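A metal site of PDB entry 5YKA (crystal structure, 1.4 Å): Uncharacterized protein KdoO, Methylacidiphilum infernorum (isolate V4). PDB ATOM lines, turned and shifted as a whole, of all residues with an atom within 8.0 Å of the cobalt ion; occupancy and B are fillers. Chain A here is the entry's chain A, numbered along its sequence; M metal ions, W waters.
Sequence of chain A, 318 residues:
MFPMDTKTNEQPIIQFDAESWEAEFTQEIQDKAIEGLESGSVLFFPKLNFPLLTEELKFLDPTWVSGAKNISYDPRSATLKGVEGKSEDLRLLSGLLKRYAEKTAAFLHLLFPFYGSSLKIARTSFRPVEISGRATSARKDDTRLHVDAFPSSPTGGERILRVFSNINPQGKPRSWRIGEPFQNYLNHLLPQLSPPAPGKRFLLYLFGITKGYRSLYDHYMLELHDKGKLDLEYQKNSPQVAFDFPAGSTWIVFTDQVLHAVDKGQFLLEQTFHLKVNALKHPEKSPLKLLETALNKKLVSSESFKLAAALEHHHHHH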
ATOM      1  N   ARG A 127      16.691  23.081 -20.954  1.00  0.00           N
ATOM      2  CA  ARG A 127      18.011  22.521 -20.684  1.00  0.00           C
ATOM      3  C   ARG A 127      18.998  23.659 -20.474  1.00  0.00           C
ATOM      4  O   ARG A 127      19.570  24.176 -21.436  1.00  0.00           O
ATOM      5  CB  ARG A 127      18.456  21.593 -21.822  1.00  0.00           C
ATOM      6  CG  ARG A 127      17.412  20.570 -22.236  1.00  0.00           C
ATOM      7  CD  ARG A 127      17.334  19.390 -21.291  1.00  0.00           C
ATOM      8  NE  ARG A 127      16.365  18.417 -21.778  1.00  0.00           N
ATOM      9  CZ  ARG A 127      16.667  17.303 -22.429  1.00  0.00           C
ATOM     10  NH1 ARG A 127      17.943  16.992 -22.668  1.00  0.00           N
ATOM     11  NH2 ARG A 127      15.705  16.486 -22.854  1.00  0.00           N
ATOM     12  N   ASP A 142      25.773  11.511 -24.750  1.00  0.00           N
ATOM     13  CA  ASP A 142      25.192  11.968 -26.004  1.00  0.00           C
ATOM     14  C   ASP A 142      26.178  12.690 -26.916  1.00  0.00           C
ATOM     15  O   ASP A 142      25.754  13.211 -27.959  1.00  0.00           O
ATOM     16  CB  ASP A 142      23.893  12.743 -25.771  1.00  0.00           C
ATOM     17  CG  ASP A 142      22.670  11.828 -25.624  1.00  0.00           C
ATOM     18  OD1 ASP A 142      21.542  12.352 -25.575  1.00  0.00           O
ATOM     19  OD2 ASP A 142      22.845  10.593 -25.569  1.00  0.00           O
ATOM     20  N   ARG A 144      28.102  10.696 -28.255  1.00  0.00           N
ATOM     21  CA  ARG A 144      28.216   9.537 -29.127  1.00  0.00           C
ATOM     22  C   ARG A 144      26.982   9.483 -30.010  1.00  0.00           C
ATOM     23  O   ARG A 144      25.863   9.662 -29.521  1.00  0.00           O
ATOM     24  CB  ARG A 144      28.355   8.270 -28.292  1.00  0.00           C
ATOM     25  CG  ARG A 144      29.504   8.351 -27.312  1.00  0.00           C
ATOM     26  CD  ARG A 144      29.722   7.027 -26.601  1.00  0.00           C
ATOM     27  NE  ARG A 144      30.753   7.154 -25.571  1.00  0.00           N
ATOM     28  CZ  ARG A 144      31.526   6.151 -25.180  1.00  0.00           C
ATOM     29  NH1 ARG A 144      31.400   4.965 -25.754  1.00  0.00           N
ATOM     30  NH2 ARG A 144      32.437   6.341 -24.236  1.00  0.00           N
ATOM     31  N   LEU A 145      27.195   9.262 -31.301  1.00  0.00           N
ATOM     32  CA  LEU A 145      26.100   9.198 -32.255  1.00  0.00           C
ATOM     33  C   LEU A 145      25.110   8.108 -31.864  1.00  0.00           C
ATOM     34  O   LEU A 145      25.510   7.004 -31.496  1.00  0.00           O
ATOM     35  CB  LEU A 145      26.661   8.864 -33.649  1.00  0.00           C
ATOM     36  CG  LEU A 145      27.514   9.933 -34.337  1.00  0.00           C
ATOM     37  CD1 LEU A 145      28.285   9.285 -35.481  1.00  0.00           C
ATOM     38  CD2 LEU A 145      26.621  11.072 -34.825  1.00  0.00           C
ATOM     39  N   HIS A 146      23.824   8.434 -31.961  1.00  0.00           N
ATOM     40  CA  HIS A 146      22.776   7.496 -31.583  1.00  0.00           C
ATOM     41  C   HIS A 146      21.476   7.946 -32.236  1.00  0.00           C
ATOM     42  O   HIS A 146      21.325   9.092 -32.675  1.00  0.00           O
ATOM     43  CB  HIS A 146      22.592   7.496 -30.050  1.00  0.00           C
ATOM     44  CG  HIS A 146      22.149   8.824 -29.516  1.00  0.00           C
ATOM     45  ND1 HIS A 146      23.007   9.884 -29.335  1.00  0.00           N
ATOM     46  CD2 HIS A 146      20.913   9.282 -29.189  1.00  0.00           C
ATOM     47  CE1 HIS A 146      22.321  10.935 -28.910  1.00  0.00           C
ATOM     48  NE2 HIS A 146      21.055  10.584 -28.798  1.00  0.00           N
ATOM     49  N   VAL A 147      20.516   7.024 -32.285  1.00  0.00           N
ATOM     50  CA  VAL A 147      19.114   7.383 -32.387  1.00  0.00           C
ATOM     51  C   VAL A 147      18.516   7.280 -30.988  1.00  0.00           C
ATOM     52  O   VAL A 147      19.027   6.584 -30.112  1.00  0.00           O
ATOM     53  CB  VAL A 147      18.318   6.513 -33.377  1.00  0.00           C
ATOM     54  CG1 VAL A 147      18.875   6.680 -34.784  1.00  0.00           C
ATOM     55  CG2 VAL A 147      18.366   5.053 -32.959  1.00  0.00           C
ATOM     56  N   ASP A 148      17.422   8.016 -30.769  1.00  0.00           N
ATOM     57  CA  ASP A 148      16.825   8.099 -29.436  1.00  0.00           C
ATOM     58  C   ASP A 148      16.027   6.848 -29.110  1.00  0.00           C
ATOM     59  O   ASP A 148      15.200   6.388 -29.903  1.00  0.00           O
ATOM     60  CB  ASP A 148      15.910   9.322 -29.311  1.00  0.00           C
ATOM     61  CG  ASP A 148      16.693  10.600 -29.157  1.00  0.00           C
ATOM     62  OD1 ASP A 148      17.951  10.553 -29.084  1.00  0.00           O
ATOM     63  OD2 ASP A 148      16.061  11.679 -29.090  1.00  0.00           O
ATOM     64  N   ALA A 149      16.295   6.303 -27.924  1.00  0.00           N
ATOM     65  CA  ALA A 149      15.576   5.182 -27.377  1.00  0.00           C
ATOM     66  C   ALA A 149      15.782   5.267 -25.875  1.00  0.00           C
ATOM     67  O   ALA A 149      16.913   5.443 -25.429  1.00  0.00           O
ATOM     68  CB  ALA A 149      16.161   3.865 -27.904  1.00  0.00           C
ATOM     69  N   PHE A 150      14.694   5.194 -25.114  1.00  0.00           N
ATOM     70  CA  PHE A 150      14.752   5.434 -23.685  1.00  0.00           C
ATOM     71  C   PHE A 150      14.348   4.175 -22.937  1.00  0.00           C
ATOM     72  O   PHE A 150      13.199   3.721 -23.078  1.00  0.00           O
ATOM     73  CB  PHE A 150      13.854   6.628 -23.322  1.00  0.00           C
ATOM     74  CG  PHE A 150      14.228   7.864 -24.065  1.00  0.00           C
ATOM     75  CD1 PHE A 150      15.381   8.562 -23.737  1.00  0.00           C
ATOM     76  CD2 PHE A 150      13.481   8.300 -25.141  1.00  0.00           C
ATOM     77  CE1 PHE A 150      15.747   9.697 -24.453  1.00  0.00           C
ATOM     78  CE2 PHE A 150      13.838   9.438 -25.851  1.00  0.00           C
ATOM     79  CZ  PHE A 150      14.980  10.129 -25.503  1.00  0.00           C
ATOM     80  N   ARG A 162      11.021  15.723 -32.476  1.00  0.00           N
ATOM     81  CA  ARG A 162      11.423  16.766 -31.556  1.00  0.00           C
ATOM     82  C   ARG A 162      11.657  18.096 -32.260  1.00  0.00           C
ATOM     83  O   ARG A 162      12.209  18.147 -33.376  1.00  0.00           O
ATOM     84  CB  ARG A 162      12.641  16.355 -30.728  1.00  0.00           C
ATOM     85  CG  ARG A 162      12.259  15.274 -29.717  1.00  0.00           C
ATOM     86  CD  ARG A 162      13.435  14.728 -28.921  1.00  0.00           C
ATOM     87  NE  ARG A 162      13.020  14.426 -27.550  1.00  0.00           N
ATOM     88  CZ  ARG A 162      13.797  13.873 -26.635  1.00  0.00           C
ATOM     89  NH1 ARG A 162      15.034  13.530 -26.940  1.00  0.00           N
ATOM     90  NH2 ARG A 162      13.334  13.654 -25.416  1.00  0.00           N
ATOM     91  N   PHE A 164      13.491  21.825 -31.490  1.00  0.00           N
ATOM     92  CA  PHE A 164      14.550  22.386 -30.666  1.00  0.00           C
ATOM     93  C   PHE A 164      14.710  23.873 -30.958  1.00  0.00           C
ATOM     94  O   PHE A 164      14.676  24.289 -32.122  1.00  0.00           O
ATOM     95  CB  PHE A 164      15.902  21.748 -31.029  1.00  0.00           C
ATOM     96  CG  PHE A 164      15.983  20.253 -30.798  1.00  0.00           C
ATOM     97  CD1 PHE A 164      15.562  19.360 -31.764  1.00  0.00           C
ATOM     98  CD2 PHE A 164      16.518  19.756 -29.618  1.00  0.00           C
ATOM     99  CE1 PHE A 164      15.678  17.979 -31.551  1.00  0.00           C
ATOM    100  CE2 PHE A 164      16.625  18.367 -29.412  1.00  0.00           C
ATOM    101  CZ  PHE A 164      16.209  17.493 -30.379  1.00  0.00           C
ATOM    102  N   TRP A 176      26.113  20.186 -32.990  1.00  0.00           N
ATOM    103  CA  TRP A 176      25.696  18.812 -33.218  1.00  0.00           C
ATOM    104  C   TRP A 176      26.616  18.146 -34.226  1.00  0.00           C
ATOM    105  O   TRP A 176      27.322  18.797 -34.998  1.00  0.00           O
ATOM    106  CB  TRP A 176      24.281  18.756 -33.805  1.00  0.00           C
ATOM    107  CG  TRP A 176      23.155  18.814 -32.834  1.00  0.00           C
ATOM    108  CD1 TRP A 176      23.120  19.490 -31.643  1.00  0.00           C
ATOM    109  CD2 TRP A 176      21.891  18.164 -32.976  1.00  0.00           C
ATOM    110  NE1 TRP A 176      21.887  19.289 -31.038  1.00  0.00           N
ATOM    111  CE2 TRP A 176      21.123  18.477 -31.835  1.00  0.00           C
ATOM    112  CE3 TRP A 176      21.333  17.330 -33.951  1.00  0.00           C
ATOM    113  CZ2 TRP A 176      19.823  17.982 -31.648  1.00  0.00           C
ATOM    114  CZ3 TRP A 176      20.039  16.854 -33.764  1.00  0.00           C
ATOM    115  CH2 TRP A 176      19.305  17.189 -32.621  1.00  0.00           C
ATOM    116  N   HIS A 225      21.001   1.830 -30.173  1.00  0.00           N
ATOM    117  CA  HIS A 225      21.453   2.950 -29.379  1.00  0.00           C
ATOM    118  C   HIS A 225      22.681   2.577 -28.538  1.00  0.00           C
ATOM    119  O   HIS A 225      23.694   3.189 -28.631  1.00  0.00           O
ATOM    120  CB  HIS A 225      20.273   3.479 -28.503  1.00  0.00           C
ATOM    121  CG  HIS A 225      20.659   4.448 -27.430  1.00  0.00           C
ATOM    122  ND1 HIS A 225      20.338   5.778 -27.454  1.00  0.00           N
ATOM    123  CD2 HIS A 225      21.300   4.243 -26.263  1.00  0.00           C
ATOM    124  CE1 HIS A 225      20.805   6.360 -26.367  1.00  0.00           C
ATOM    125  NE2 HIS A 225      21.379   5.444 -25.623  1.00  0.00           N
ATOM    126  N   LYS A 229      26.789   3.203 -29.511  1.00  0.00           N
ATOM    127  CA  LYS A 229      27.612   4.081 -28.670  1.00  0.00           C
ATOM    128  C   LYS A 229      28.888   3.394 -28.212  1.00  0.00           C
ATOM    129  O   LYS A 229      29.909   4.063 -28.031  1.00  0.00           O
ATOM    130  CB  LYS A 229      26.803   4.565 -27.464  1.00  0.00           C
ATOM    131  CG  LYS A 229      25.751   5.597 -27.797  1.00  0.00           C
ATOM    132  CD  LYS A 229      25.199   6.227 -26.532  1.00  0.00           C
ATOM    133  CE  LYS A 229      24.322   7.418 -26.844  1.00  0.00           C
ATOM    134  NZ  LYS A 229      23.987   8.151 -25.599  1.00  0.00           N
ATOM    135  N   THR A 255      14.181  12.128 -34.073  1.00  0.00           N
ATOM    136  CA  THR A 255      15.364  11.724 -33.370  1.00  0.00           C
ATOM    137  C   THR A 255      15.553  10.248 -33.194  1.00  0.00           C
ATOM    138  O   THR A 255      16.576   9.871 -32.785  1.00  0.00           O
ATOM    139  CB  THR A 255      15.547  12.446 -32.033  1.00  0.00           C
ATOM    140  OG1 THR A 255      14.430  12.185 -31.221  1.00  0.00           O
ATOM    141  CG2 THR A 255      15.713  13.964 -32.234  1.00  0.00           C
ATOM    142  N   ASP A 256      14.532   9.491 -33.535  1.00  0.00           N
ATOM    143  CA  ASP A 256      14.614   8.052 -33.563  1.00  0.00           C
ATOM    144  C   ASP A 256      15.135   7.543 -34.908  1.00  0.00           C
ATOM    145  O   ASP A 256      15.307   6.386 -35.093  1.00  0.00           O
ATOM    146  CB  ASP A 256      13.246   7.412 -33.274  1.00  0.00           C
ATOM    147  CG  ASP A 256      12.145   7.848 -34.228  1.00  0.00           C
ATOM    148  OD1 ASP A 256      12.432   8.628 -35.082  1.00  0.00           O
ATOM    149  OD2 ASP A 256      11.029   7.393 -34.060  1.00  0.00           O
ATOM    150  N   VAL A 258      17.240  10.020 -37.211  1.00  0.00           N
ATOM    151  CA  VAL A 258      18.413  10.799 -37.525  1.00  0.00           C
ATOM    152  C   VAL A 258      19.487  10.496 -36.511  1.00  0.00           C
ATOM    153  O   VAL A 258      19.354  10.783 -35.372  1.00  0.00           O
ATOM    154  CB  VAL A 258      18.086  12.298 -37.524  1.00  0.00           C
ATOM    155  CG1 VAL A 258      19.343  13.126 -37.805  1.00  0.00           C
ATOM    156  CG2 VAL A 258      17.064  12.584 -38.582  1.00  0.00           C
ATOM    157  N   LEU A 259      20.544   9.899 -36.982  1.00  0.00           N
ATOM    158  CA  LEU A 259      21.748   9.722 -36.083  1.00  0.00           C
ATOM    159  C   LEU A 259      22.457  11.072 -35.612  1.00  0.00           C
ATOM    160  O   LEU A 259      22.625  11.875 -36.472  1.00  0.00           O
ATOM    161  CB  LEU A 259      22.820   8.915 -36.827  1.00  0.00           C
ATOM    162  CG  LEU A 259      22.694   7.391 -36.799  1.00  0.00           C
ATOM    163  CD1 LEU A 259      21.453   6.927 -37.539  1.00  0.00           C
ATOM    164  CD2 LEU A 259      23.948   6.786 -37.401  1.00  0.00           C
ATOM    165  N   HIS A 260      22.503  11.311 -34.340  1.00  0.00           N
ATOM    166  CA  HIS A 260      22.948  12.579 -33.897  1.00  0.00           C
ATOM    167  C   HIS A 260      23.772  12.459 -32.638  1.00  0.00           C
ATOM    168  O   HIS A 260      23.731  11.479 -31.978  1.00  0.00           O
ATOM    169  CB  HIS A 260      21.714  13.502 -33.673  1.00  0.00           C
ATOM    170  CG  HIS A 260      20.786  12.985 -32.624  1.00  0.00           C
ATOM    171  ND1 HIS A 260      19.875  11.981 -32.855  1.00  0.00           N
ATOM    172  CD2 HIS A 260      20.674  13.281 -31.320  1.00  0.00           C
ATOM    173  CE1 HIS A 260      19.251  11.701 -31.740  1.00  0.00           C
ATOM    174  NE2 HIS A 260      19.715  12.478 -30.792  1.00  0.00           N
ATOM    175  N   ALA A 261      24.518  13.510 -32.397  1.00  0.00           N
ATOM    176  CA  ALA A 261      25.310  13.689 -31.207  1.00  0.00           C
ATOM    177  C   ALA A 261      25.364  15.170 -30.891  1.00  0.00           C
ATOM    178  O   ALA A 261      25.289  15.949 -31.758  1.00  0.00           O
ATOM    179  CB  ALA A 261      26.732  13.120 -31.354  1.00  0.00           C
ATOM    180  N   VAL A 262      25.499  15.488 -29.622  1.00  0.00           N
ATOM    181  CA  VAL A 262      25.568  16.855 -29.134  1.00  0.00           C
ATOM    182  C   VAL A 262      26.889  17.098 -28.424  1.00  0.00           C
ATOM    183  O   VAL A 262      27.206  16.427 -27.533  1.00  0.00           O
ATOM    184  CB  VAL A 262      24.395  17.164 -28.231  1.00  0.00           C
ATOM    185  CG1 VAL A 262      24.303  18.653 -28.043  1.00  0.00           C
ATOM    186  CG2 VAL A 262      23.104  16.676 -28.847  1.00  0.00           C
ATOM    187  N   GLU A 270      13.105  22.358 -25.822  1.00  0.00           N
ATOM    188  CA  GLU A 270      12.876  21.185 -26.634  1.00  0.00           C
ATOM    189  C   GLU A 270      11.452  20.716 -26.396  1.00  0.00           C
ATOM    190  O   GLU A 270      10.954  20.785 -25.259  1.00  0.00           O
ATOM    191  CB  GLU A 270      13.875  20.076 -26.223  1.00  0.00           C
ATOM    192  CG  GLU A 270      13.807  18.754 -26.934  1.00  0.00           C
ATOM    193  CD  GLU A 270      14.990  17.873 -26.532  1.00  0.00           C
ATOM    194  OE1 GLU A 270      15.859  18.362 -25.778  1.00  0.00           O
ATOM    195  OE2 GLU A 270      15.072  16.714 -26.981  1.00  0.00           O
HETATM  196 CO    CO M   1      19.444  12.008 -28.679  1.00  0.00          CO
HETATM  197  O   HOH W   1      17.917  13.482 -28.527  1.00  0.00           O
HETATM  198  O   HOH W   2      19.157  11.479 -26.644  1.00  0.00           O
HETATM  199  O   HOH W   3      20.795  13.604 -28.033  1.00  0.00           O
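Water W2 binds the cobalt ion (2.1 Å). OD1 of Asp 148 binds the cobalt ion (2.1 Å). Water W1 binds the cobalt ion. NE2 of His 146 binds the cobalt ion (2.2 Å). NE2 of His 260 is bound to the cobalt ion, at 2.2 Å. Water W3 binds the cobalt ion (2.2 Å).
Water W1 bridges the side-chain carboxylate (OD2) of Asp 148 and the guanidinium group (NH1) of Arg 162.
OD1 of Asp 142 touches the cobalt ion, 3.8 Å away. Along chain A the residues within 4 Å of the cobalt ion span positions 142 to 260.
OD2 of Asp 148 is in salt-bridge range of NH1 of Arg 162 (3.0 Å). OD2 of Asp 148 lies within hydrogen-bond range of OG1 of Thr 255. A ring nitrogen (ND1) of His 146 is in hydrogen-bond range of the backbone carbonyl oxygen of Arg 144 (2.9 Å). ND1 of His 260 is in hydrogen-bond range of O of Val 258 (2.8 Å). The backbone carbonyl oxygen (O) of Asp 142 is in hydrogen-bond range of the backbone NH (N) of Val 262, 2.8 Å away. The side-chain carboxylate (OD2) of Asp 142 lies within salt-bridge range of the side-chain amino group (NZ) of Lys 229, at 2.7 Å.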
